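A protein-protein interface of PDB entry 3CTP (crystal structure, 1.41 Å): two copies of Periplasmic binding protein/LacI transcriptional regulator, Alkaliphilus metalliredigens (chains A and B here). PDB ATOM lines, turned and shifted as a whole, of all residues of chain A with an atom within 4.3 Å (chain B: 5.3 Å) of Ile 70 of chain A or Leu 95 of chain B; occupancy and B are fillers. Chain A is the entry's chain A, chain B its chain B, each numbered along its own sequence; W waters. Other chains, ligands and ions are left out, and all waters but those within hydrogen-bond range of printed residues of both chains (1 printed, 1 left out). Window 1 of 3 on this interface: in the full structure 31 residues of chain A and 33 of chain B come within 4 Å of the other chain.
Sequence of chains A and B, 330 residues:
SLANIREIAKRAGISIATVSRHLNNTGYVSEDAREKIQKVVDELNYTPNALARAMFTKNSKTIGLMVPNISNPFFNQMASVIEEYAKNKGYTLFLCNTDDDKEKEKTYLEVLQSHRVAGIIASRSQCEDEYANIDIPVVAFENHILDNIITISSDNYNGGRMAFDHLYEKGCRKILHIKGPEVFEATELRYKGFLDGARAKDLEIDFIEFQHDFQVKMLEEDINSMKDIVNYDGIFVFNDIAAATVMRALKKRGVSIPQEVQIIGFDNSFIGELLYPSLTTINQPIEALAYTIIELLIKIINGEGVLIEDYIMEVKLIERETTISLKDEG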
ATOM      1  N   VAL A  67     -24.671  -9.730   7.089  1.00  0.00           N
ATOM      2  CA  VAL A  67     -24.454 -11.019   6.516  1.00  0.00           C
ATOM      3  C   VAL A  67     -25.446 -12.011   7.180  1.00  0.00           C
ATOM      4  O   VAL A  67     -25.429 -12.144   8.393  1.00  0.00           O
ATOM      5  CB  VAL A  67     -22.993 -11.457   6.899  1.00  0.00           C
ATOM      6  CG1 VAL A  67     -22.624 -12.715   6.246  1.00  0.00           C
ATOM      7  CG2 VAL A  67     -21.967 -10.353   6.520  1.00  0.00           C
ATOM      8  N   ASN A  69     -25.360 -15.637   7.308  1.00  0.00           N
ATOM      9  CA  ASN A  69     -24.171 -16.143   8.019  1.00  0.00           C
ATOM     10  C   ASN A  69     -23.016 -16.438   7.132  1.00  0.00           C
ATOM     11  O   ASN A  69     -23.174 -16.949   6.025  1.00  0.00           O
ATOM     12  CB  ASN A  69     -24.473 -17.320   8.955  1.00  0.00           C
ATOM     13  CG  ASN A  69     -23.474 -17.405  10.089  1.00  0.00           C
ATOM     14  OD1 ASN A  69     -22.337 -17.825   9.901  1.00  0.00           O
ATOM     15  ND2 ASN A  69     -23.873 -16.943  11.262  1.00  0.00           N
ATOM     16  N   ILE A  70     -21.832 -16.054   7.609  1.00  0.00           N
ATOM     17  CA  ILE A  70     -20.595 -16.239   6.802  1.00  0.00           C
ATOM     18  C   ILE A  70     -20.188 -17.702   6.799  1.00  0.00           C
ATOM     19  O   ILE A  70     -19.278 -18.105   6.032  1.00  0.00           O
ATOM     20  CB  ILE A  70     -19.370 -15.378   7.250  1.00  0.00           C
ATOM     21  CG1 ILE A  70     -19.085 -15.555   8.739  1.00  0.00           C
ATOM     22  CG2 ILE A  70     -19.559 -13.896   6.842  1.00  0.00           C
ATOM     23  CD1 ILE A  70     -17.793 -14.904   9.204  1.00  0.00           C
ATOM     24  N   SER A  71     -20.888 -18.492   7.608  1.00  0.00           N
ATOM     25  CA  SER A  71     -20.806 -19.987   7.443  1.00  0.00           C
ATOM     26  C   SER A  71     -21.278 -20.527   6.096  1.00  0.00           C
ATOM     27  O   SER A  71     -20.868 -21.610   5.684  1.00  0.00           O
ATOM     28  CB  SER A  71     -21.519 -20.755   8.526  1.00  0.00           C
ATOM     29  OG  SER A  71     -22.905 -20.878   8.269  1.00  0.00           O
ATOM     30  N   ASN A  72     -22.097 -19.764   5.383  1.00  0.00           N
ATOM     31  CA  ASN A  72     -22.369 -20.113   3.976  1.00  0.00           C
ATOM     32  C   ASN A  72     -21.262 -19.533   3.100  1.00  0.00           C
ATOM     33  O   ASN A  72     -21.046 -18.318   3.101  1.00  0.00           O
ATOM     34  CB  ASN A  72     -23.739 -19.520   3.604  1.00  0.00           C
ATOM     35  CG  ASN A  72     -24.114 -19.787   2.166  1.00  0.00           C
ATOM     36  OD1 ASN A  72     -23.266 -20.129   1.318  1.00  0.00           O
ATOM     37  ND2 ASN A  72     -25.422 -19.647   1.870  1.00  0.00           N
ATOM     38  N   ASN A  76     -19.410 -15.603   2.717  1.00  0.00           N
ATOM     39  CA  ASN A  76     -18.052 -15.164   3.056  1.00  0.00           C
ATOM     40  C   ASN A  76     -17.280 -14.703   1.829  1.00  0.00           C
ATOM     41  O   ASN A  76     -16.478 -13.772   1.908  1.00  0.00           O
ATOM     42  CB  ASN A  76     -17.287 -16.131   3.972  1.00  0.00           C
ATOM     43  CG  ASN A  76     -17.041 -17.484   3.382  1.00  0.00           C
ATOM     44  OD1 ASN A  76     -16.315 -17.595   2.381  1.00  0.00           O
ATOM     45  ND2 ASN A  76     -17.512 -18.571   4.085  1.00  0.00           N
ATOM     46  N   PHE A  94     -17.463  -3.281   8.740  1.00  0.00           N
ATOM     47  CA  PHE A  94     -17.804  -4.101   9.909  1.00  0.00           C
ATOM     48  C   PHE A  94     -18.781  -5.151   9.409  1.00  0.00           C
ATOM     49  O   PHE A  94     -19.777  -4.797   8.766  1.00  0.00           O
ATOM     50  CB  PHE A  94     -18.530  -3.275  10.970  1.00  0.00           C
ATOM     51  CG  PHE A  94     -17.655  -2.316  11.733  1.00  0.00           C
ATOM     52  CD1 PHE A  94     -16.336  -2.604  11.968  1.00  0.00           C
ATOM     53  CD2 PHE A  94     -18.193  -1.165  12.262  1.00  0.00           C
ATOM     54  CE1 PHE A  94     -15.524  -1.715  12.704  1.00  0.00           C
ATOM     55  CE2 PHE A  94     -17.414  -0.298  12.988  1.00  0.00           C
ATOM     56  CZ  PHE A  94     -16.087  -0.558  13.195  1.00  0.00           C
ATOM     57  N   LEU A  95     -18.539  -6.428   9.684  1.00  0.00           N
ATOM     58  CA  LEU A  95     -19.500  -7.468   9.304  1.00  0.00           C
ATOM     59  C   LEU A  95     -20.375  -7.800  10.485  1.00  0.00           C
ATOM     60  O   LEU A  95     -19.879  -7.925  11.608  1.00  0.00           O
ATOM     61  CB  LEU A  95     -18.806  -8.760   8.887  1.00  0.00           C
ATOM     62  CG  LEU A  95     -17.665  -8.655   7.910  1.00  0.00           C
ATOM     63  CD1 LEU A  95     -17.234 -10.112   7.549  1.00  0.00           C
ATOM     64  CD2 LEU A  95     -18.128  -7.932   6.679  1.00  0.00           C
ATOM     65  N   LEU B  65     -14.406  -8.317  17.045  1.00  0.00           N
ATOM     66  CA  LEU B  65     -13.746  -9.614  16.914  1.00  0.00           C
ATOM     67  C   LEU B  65     -12.962  -9.617  15.610  1.00  0.00           C
ATOM     68  O   LEU B  65     -13.553  -9.543  14.528  1.00  0.00           O
ATOM     69  CB  LEU B  65     -14.766 -10.770  16.919  1.00  0.00           C
ATOM     70  CG  LEU B  65     -14.249 -12.152  16.483  1.00  0.00           C
ATOM     71  CD1 LEU B  65     -13.111 -12.618  17.430  1.00  0.00           C
ATOM     72  CD2 LEU B  65     -15.382 -13.183  16.471  1.00  0.00           C
ATOM     73  N   VAL B  67     -11.141 -11.436  12.794  1.00  0.00           N
ATOM     74  CA  VAL B  67     -11.283 -12.746  12.215  1.00  0.00           C
ATOM     75  C   VAL B  67     -10.235 -12.865  11.081  1.00  0.00           C
ATOM     76  O   VAL B  67     -10.288 -12.136  10.118  1.00  0.00           O
ATOM     77  CB  VAL B  67     -12.711 -12.915  11.590  1.00  0.00           C
ATOM     78  CG1 VAL B  67     -12.904 -14.313  11.111  1.00  0.00           C
ATOM     79  CG2 VAL B  67     -13.814 -12.581  12.633  1.00  0.00           C
ATOM     80  N   ILE B  70     -12.137 -15.331   7.117  1.00  0.00           N
ATOM     81  CA  ILE B  70     -13.581 -15.508   7.090  1.00  0.00           C
ATOM     82  C   ILE B  70     -13.987 -16.688   6.132  1.00  0.00           C
ATOM     83  O   ILE B  70     -15.108 -17.133   6.153  1.00  0.00           O
ATOM     84  CB  ILE B  70     -14.256 -14.153   6.743  1.00  0.00           C
ATOM     85  CG1 ILE B  70     -14.033 -13.800   5.273  1.00  0.00           C
ATOM     86  CG2 ILE B  70     -13.692 -12.983   7.679  1.00  0.00           C
ATOM     87  CD1 ILE B  70     -15.123 -12.895   4.698  1.00  0.00           C
ATOM     88  N   ASN B  76     -15.698 -19.218  11.134  1.00  0.00           N
ATOM     89  CA  ASN B  76     -17.126 -18.846  11.106  1.00  0.00           C
ATOM     90  C   ASN B  76     -17.827 -19.457  12.326  1.00  0.00           C
ATOM     91  O   ASN B  76     -18.692 -18.820  12.948  1.00  0.00           O
ATOM     92  CB  ASN B  76     -17.911 -19.384   9.886  1.00  0.00           C
ATOM     93  CG  ASN B  76     -17.184 -19.309   8.596  1.00  0.00           C
ATOM     94  OD1 ASN B  76     -17.258 -20.254   7.781  1.00  0.00           O
ATOM     95  ND2 ASN B  76     -16.560 -18.172   8.334  1.00  0.00           N
ATOM     96  N   ALA B  79     -16.849 -17.529  15.430  1.00  0.00           N
ATOM     97  CA  ALA B  79     -17.515 -16.224  15.515  1.00  0.00           C
ATOM     98  C   ALA B  79     -18.955 -16.381  15.965  1.00  0.00           C
ATOM     99  O   ALA B  79     -19.460 -15.549  16.726  1.00  0.00           O
ATOM    100  CB  ALA B  79     -17.449 -15.500  14.160  1.00  0.00           C
ATOM    101  N   GLU B  83     -20.310 -14.902  19.540  1.00  0.00           N
ATOM    102  CA  GLU B  83     -21.441 -13.988  19.550  1.00  0.00           C
ATOM    103  C   GLU B  83     -22.471 -14.398  20.602  1.00  0.00           C
ATOM    104  O   GLU B  83     -23.016 -13.533  21.309  1.00  0.00           O
ATOM    105  CB  GLU B  83     -22.079 -13.886  18.158  1.00  0.00           C
ATOM    106  CG  GLU B  83     -23.308 -12.976  18.182  1.00  0.00           C
ATOM    107  CD  GLU B  83     -23.325 -11.950  17.077  1.00  0.00           C
ATOM    108  OE1 GLU B  83     -22.329 -11.852  16.315  1.00  0.00           O
ATOM    109  OE2 GLU B  83     -24.333 -11.214  16.991  1.00  0.00           O
ATOM    110  N   LEU B  93     -21.355  -7.936  18.604  1.00  0.00           N
ATOM    111  CA  LEU B  93     -19.999  -8.057  18.027  1.00  0.00           C
ATOM    112  C   LEU B  93     -19.954  -7.389  16.665  1.00  0.00           C
ATOM    113  O   LEU B  93     -20.914  -7.498  15.894  1.00  0.00           O
ATOM    114  CB  LEU B  93     -19.665  -9.510  17.715  1.00  0.00           C
ATOM    115  CG  LEU B  93     -19.383 -10.553  18.768  1.00  0.00           C
ATOM    116  CD1 LEU B  93     -18.944 -11.806  18.040  1.00  0.00           C
ATOM    117  CD2 LEU B  93     -18.273 -10.065  19.664  1.00  0.00           C
ATOM    118  N   PHE B  94     -18.837  -6.750  16.356  1.00  0.00           N
ATOM    119  CA  PHE B  94     -18.515  -6.415  14.962  1.00  0.00           C
ATOM    120  C   PHE B  94     -17.436  -7.394  14.519  1.00  0.00           C
ATOM    121  O   PHE B  94     -16.419  -7.527  15.221  1.00  0.00           O
ATOM    122  CB  PHE B  94     -17.902  -5.024  14.873  1.00  0.00           C
ATOM    123  CG  PHE B  94     -18.885  -3.887  15.057  1.00  0.00           C
ATOM    124  CD1 PHE B  94     -20.191  -4.003  14.649  1.00  0.00           C
ATOM    125  CD2 PHE B  94     -18.455  -2.682  15.590  1.00  0.00           C
ATOM    126  CE1 PHE B  94     -21.096  -2.919  14.799  1.00  0.00           C
ATOM    127  CE2 PHE B  94     -19.321  -1.623  15.744  1.00  0.00           C
ATOM    128  CZ  PHE B  94     -20.645  -1.738  15.357  1.00  0.00           C
ATOM    129  N   LEU B  95     -17.587  -8.031  13.364  1.00  0.00           N
ATOM    130  CA  LEU B  95     -16.504  -8.885  12.886  1.00  0.00           C
ATOM    131  C   LEU B  95     -15.643  -8.103  11.927  1.00  0.00           C
ATOM    132  O   LEU B  95     -16.163  -7.398  11.067  1.00  0.00           O
ATOM    133  CB  LEU B  95     -17.020 -10.106  12.149  1.00  0.00           C
ATOM    134  CG  LEU B  95     -18.123 -10.893  12.830  1.00  0.00           C
ATOM    135  CD1 LEU B  95     -18.424 -12.134  11.946  1.00  0.00           C
ATOM    136  CD2 LEU B  95     -17.685 -11.315  14.209  1.00  0.00           C
ATOM    137  N   CYS B  96     -14.329  -8.252  12.053  1.00  0.00           N
ATOM    138  CA  CYS B  96     -13.387  -7.525  11.202  1.00  0.00           C
ATOM    139  C   CYS B  96     -12.474  -8.522  10.560  1.00  0.00           C
ATOM    140  O   CYS B  96     -11.794  -9.299  11.230  1.00  0.00           O
ATOM    141  CB  CYS B  96     -12.561  -6.553  12.041  1.00  0.00           C
ATOM    142  SG  CYS B  96     -13.563  -5.288  12.861  1.00  0.00           S
ATOM    143  N   ASN B  97     -12.459  -8.506   9.235  1.00  0.00           N
ATOM    144  CA  ASN B  97     -11.710  -9.440   8.467  1.00  0.00           C
ATOM    145  C   ASN B  97     -10.216  -9.042   8.338  1.00  0.00           C
ATOM    146  O   ASN B  97      -9.908  -8.114   7.612  1.00  0.00           O
ATOM    147  CB  ASN B  97     -12.318  -9.385   7.059  1.00  0.00           C
ATOM    148  CG  ASN B  97     -11.719 -10.383   6.158  1.00  0.00           C
ATOM    149  OD1 ASN B  97     -10.759 -11.037   6.520  1.00  0.00           O
ATOM    150  ND2 ASN B  97     -12.275 -10.512   4.950  1.00  0.00           N
HETATM  151  O   HOH W   1     -17.830 -21.484   5.415  1.00  0.00           O
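The side-chain amide oxygen (OD1) of Asn 76 of chain B sits close to the backbone carbonyl oxygen (O) of Ile 70 of chain A, 3.4 Å away. ND2 of Asn 76 of chain A sits close to O of Ile 70 of chain B, at 3.5 Å. The backbone carbonyl oxygen (O) of Leu 95 of chain A sits at hydrogen-bond distance from the backbone NH (N) of Leu 95 of chain B, at 2.9 Å.
OD1 of Asn 69 of chain A lies within hydrogen-bond range of N of Ser 71 of chain A, 2.8 Å away. O of Ile 70 of chain A is in hydrogen-bond range of ND2 of Asn 76 of chain A (2.7 Å). The backbone carbonyl oxygen (O) of Phe 94 of chain B is in hydrogen-bond range of the backbone NH (N) of Leu 65 of chain B (2.8 Å). The backbone NH of Cys 96 of chain B is in hydrogen-bond range of the backbone carbonyl oxygen of Leu 65 of chain B, at 2.9 Å. The backbone NH (N) of Val 67 of chain B sits at hydrogen-bond distance from the backbone carbonyl oxygen (O) of Cys 96 of chain B, at 2.7 Å. The backbone carbonyl oxygen of Ile 70 of chain B lies within hydrogen-bond range of the side-chain amide nitrogen of Asn 76 of chain B (2.8 Å).
CD1 of Ile 70 of chain A touches CD1 of Leu 95 of chain B, 3.9 Å away. OD1 of Asn 76 of chain B touches CA of Ser 71 of chain A, 3.6 Å away. Phe 94 of chain B touches Phe 94 of chain A (CE2 to CE2, 3.6 Å). Phe 94 of chain A touches Leu 95 of chain B (C to O, 3.8 Å). Cys 96 of chain B touches Phe 94 of chain A. O of Leu 95 of chain A touches C of Phe 94 of chain B, at 3.8 Å.
Of chain B, only Asn 76 and Leu 95 come within 4 Å of Ile 70 of chain A. Of the printed residues of chain B, Asn 76 of chain A touches Ile 70 (3.2 Å). Of the printed residues of chain A, Asn 76 of chain B touches Ile 70 (3.4 Å) and Ser 71 (3.6 Å). Glu 83 of chain B touches none of the printed residues of chain A. Of the printed residues of chain A, Phe 94 of chain B touches Phe 94 and Leu 95. Leu 95 of chain B touches just these residues of chain A: Ile 70, Phe 94 and Leu 95. The nearest residue of chain B that does not touch Ile 70 of chain A is Ile 70 of chain B (4.3 Å). The nearest printed residue of chain A that does not touch Leu 95 of chain B is Val 67 of chain A (6.7 Å).
Of the 11 printed residues of chain B, 5 touch a printed residue of chain A. Of the 8 printed residues of chain A, 5 touch a printed residue of chain B. Hydrophobic or aromatic side chains of chain A within 4 Å of the printed part of chain B: Ile 70, Phe 94 and Leu 95. Along chain A the printed residues that touch a printed residue of chain B span positions 70 to 95. Among the printed residues, no Asp or Glu carboxylate lies within 4 Å of a Lys or Arg side-chain nitrogen of the other chain.
Ile 70 of chain A touches Asn 76 of chain B, and with the chains exchanged Asn 76 of chain A touches Ile 70 of chain B. Ile 70 of chain A touches Leu 95 of chain B, but with the chains exchanged Leu 95 of chain A does not touch Ile 70 of chain B (4.5 Å). Phe 94 of chain B touches its own counterpart, Phe 94 of chain A. Phe 94 of chain A touches Leu 95 of chain B, and with the chains exchanged Leu 95 of chain A touches Phe 94 of chain B. Positions printed for both chains: 67, 70, 76, 94 and 95.
Water W1 lies within hydrogen-bond range of the side-chain amide oxygen (OD1) of Asn 76 of chain B (2.7 Å), the backbone carbonyl oxygen (O) of Ser 71 of chain A (3.1 Å) and the side-chain amide nitrogen (ND2) of Asn 76 of chain A (3.2 Å).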
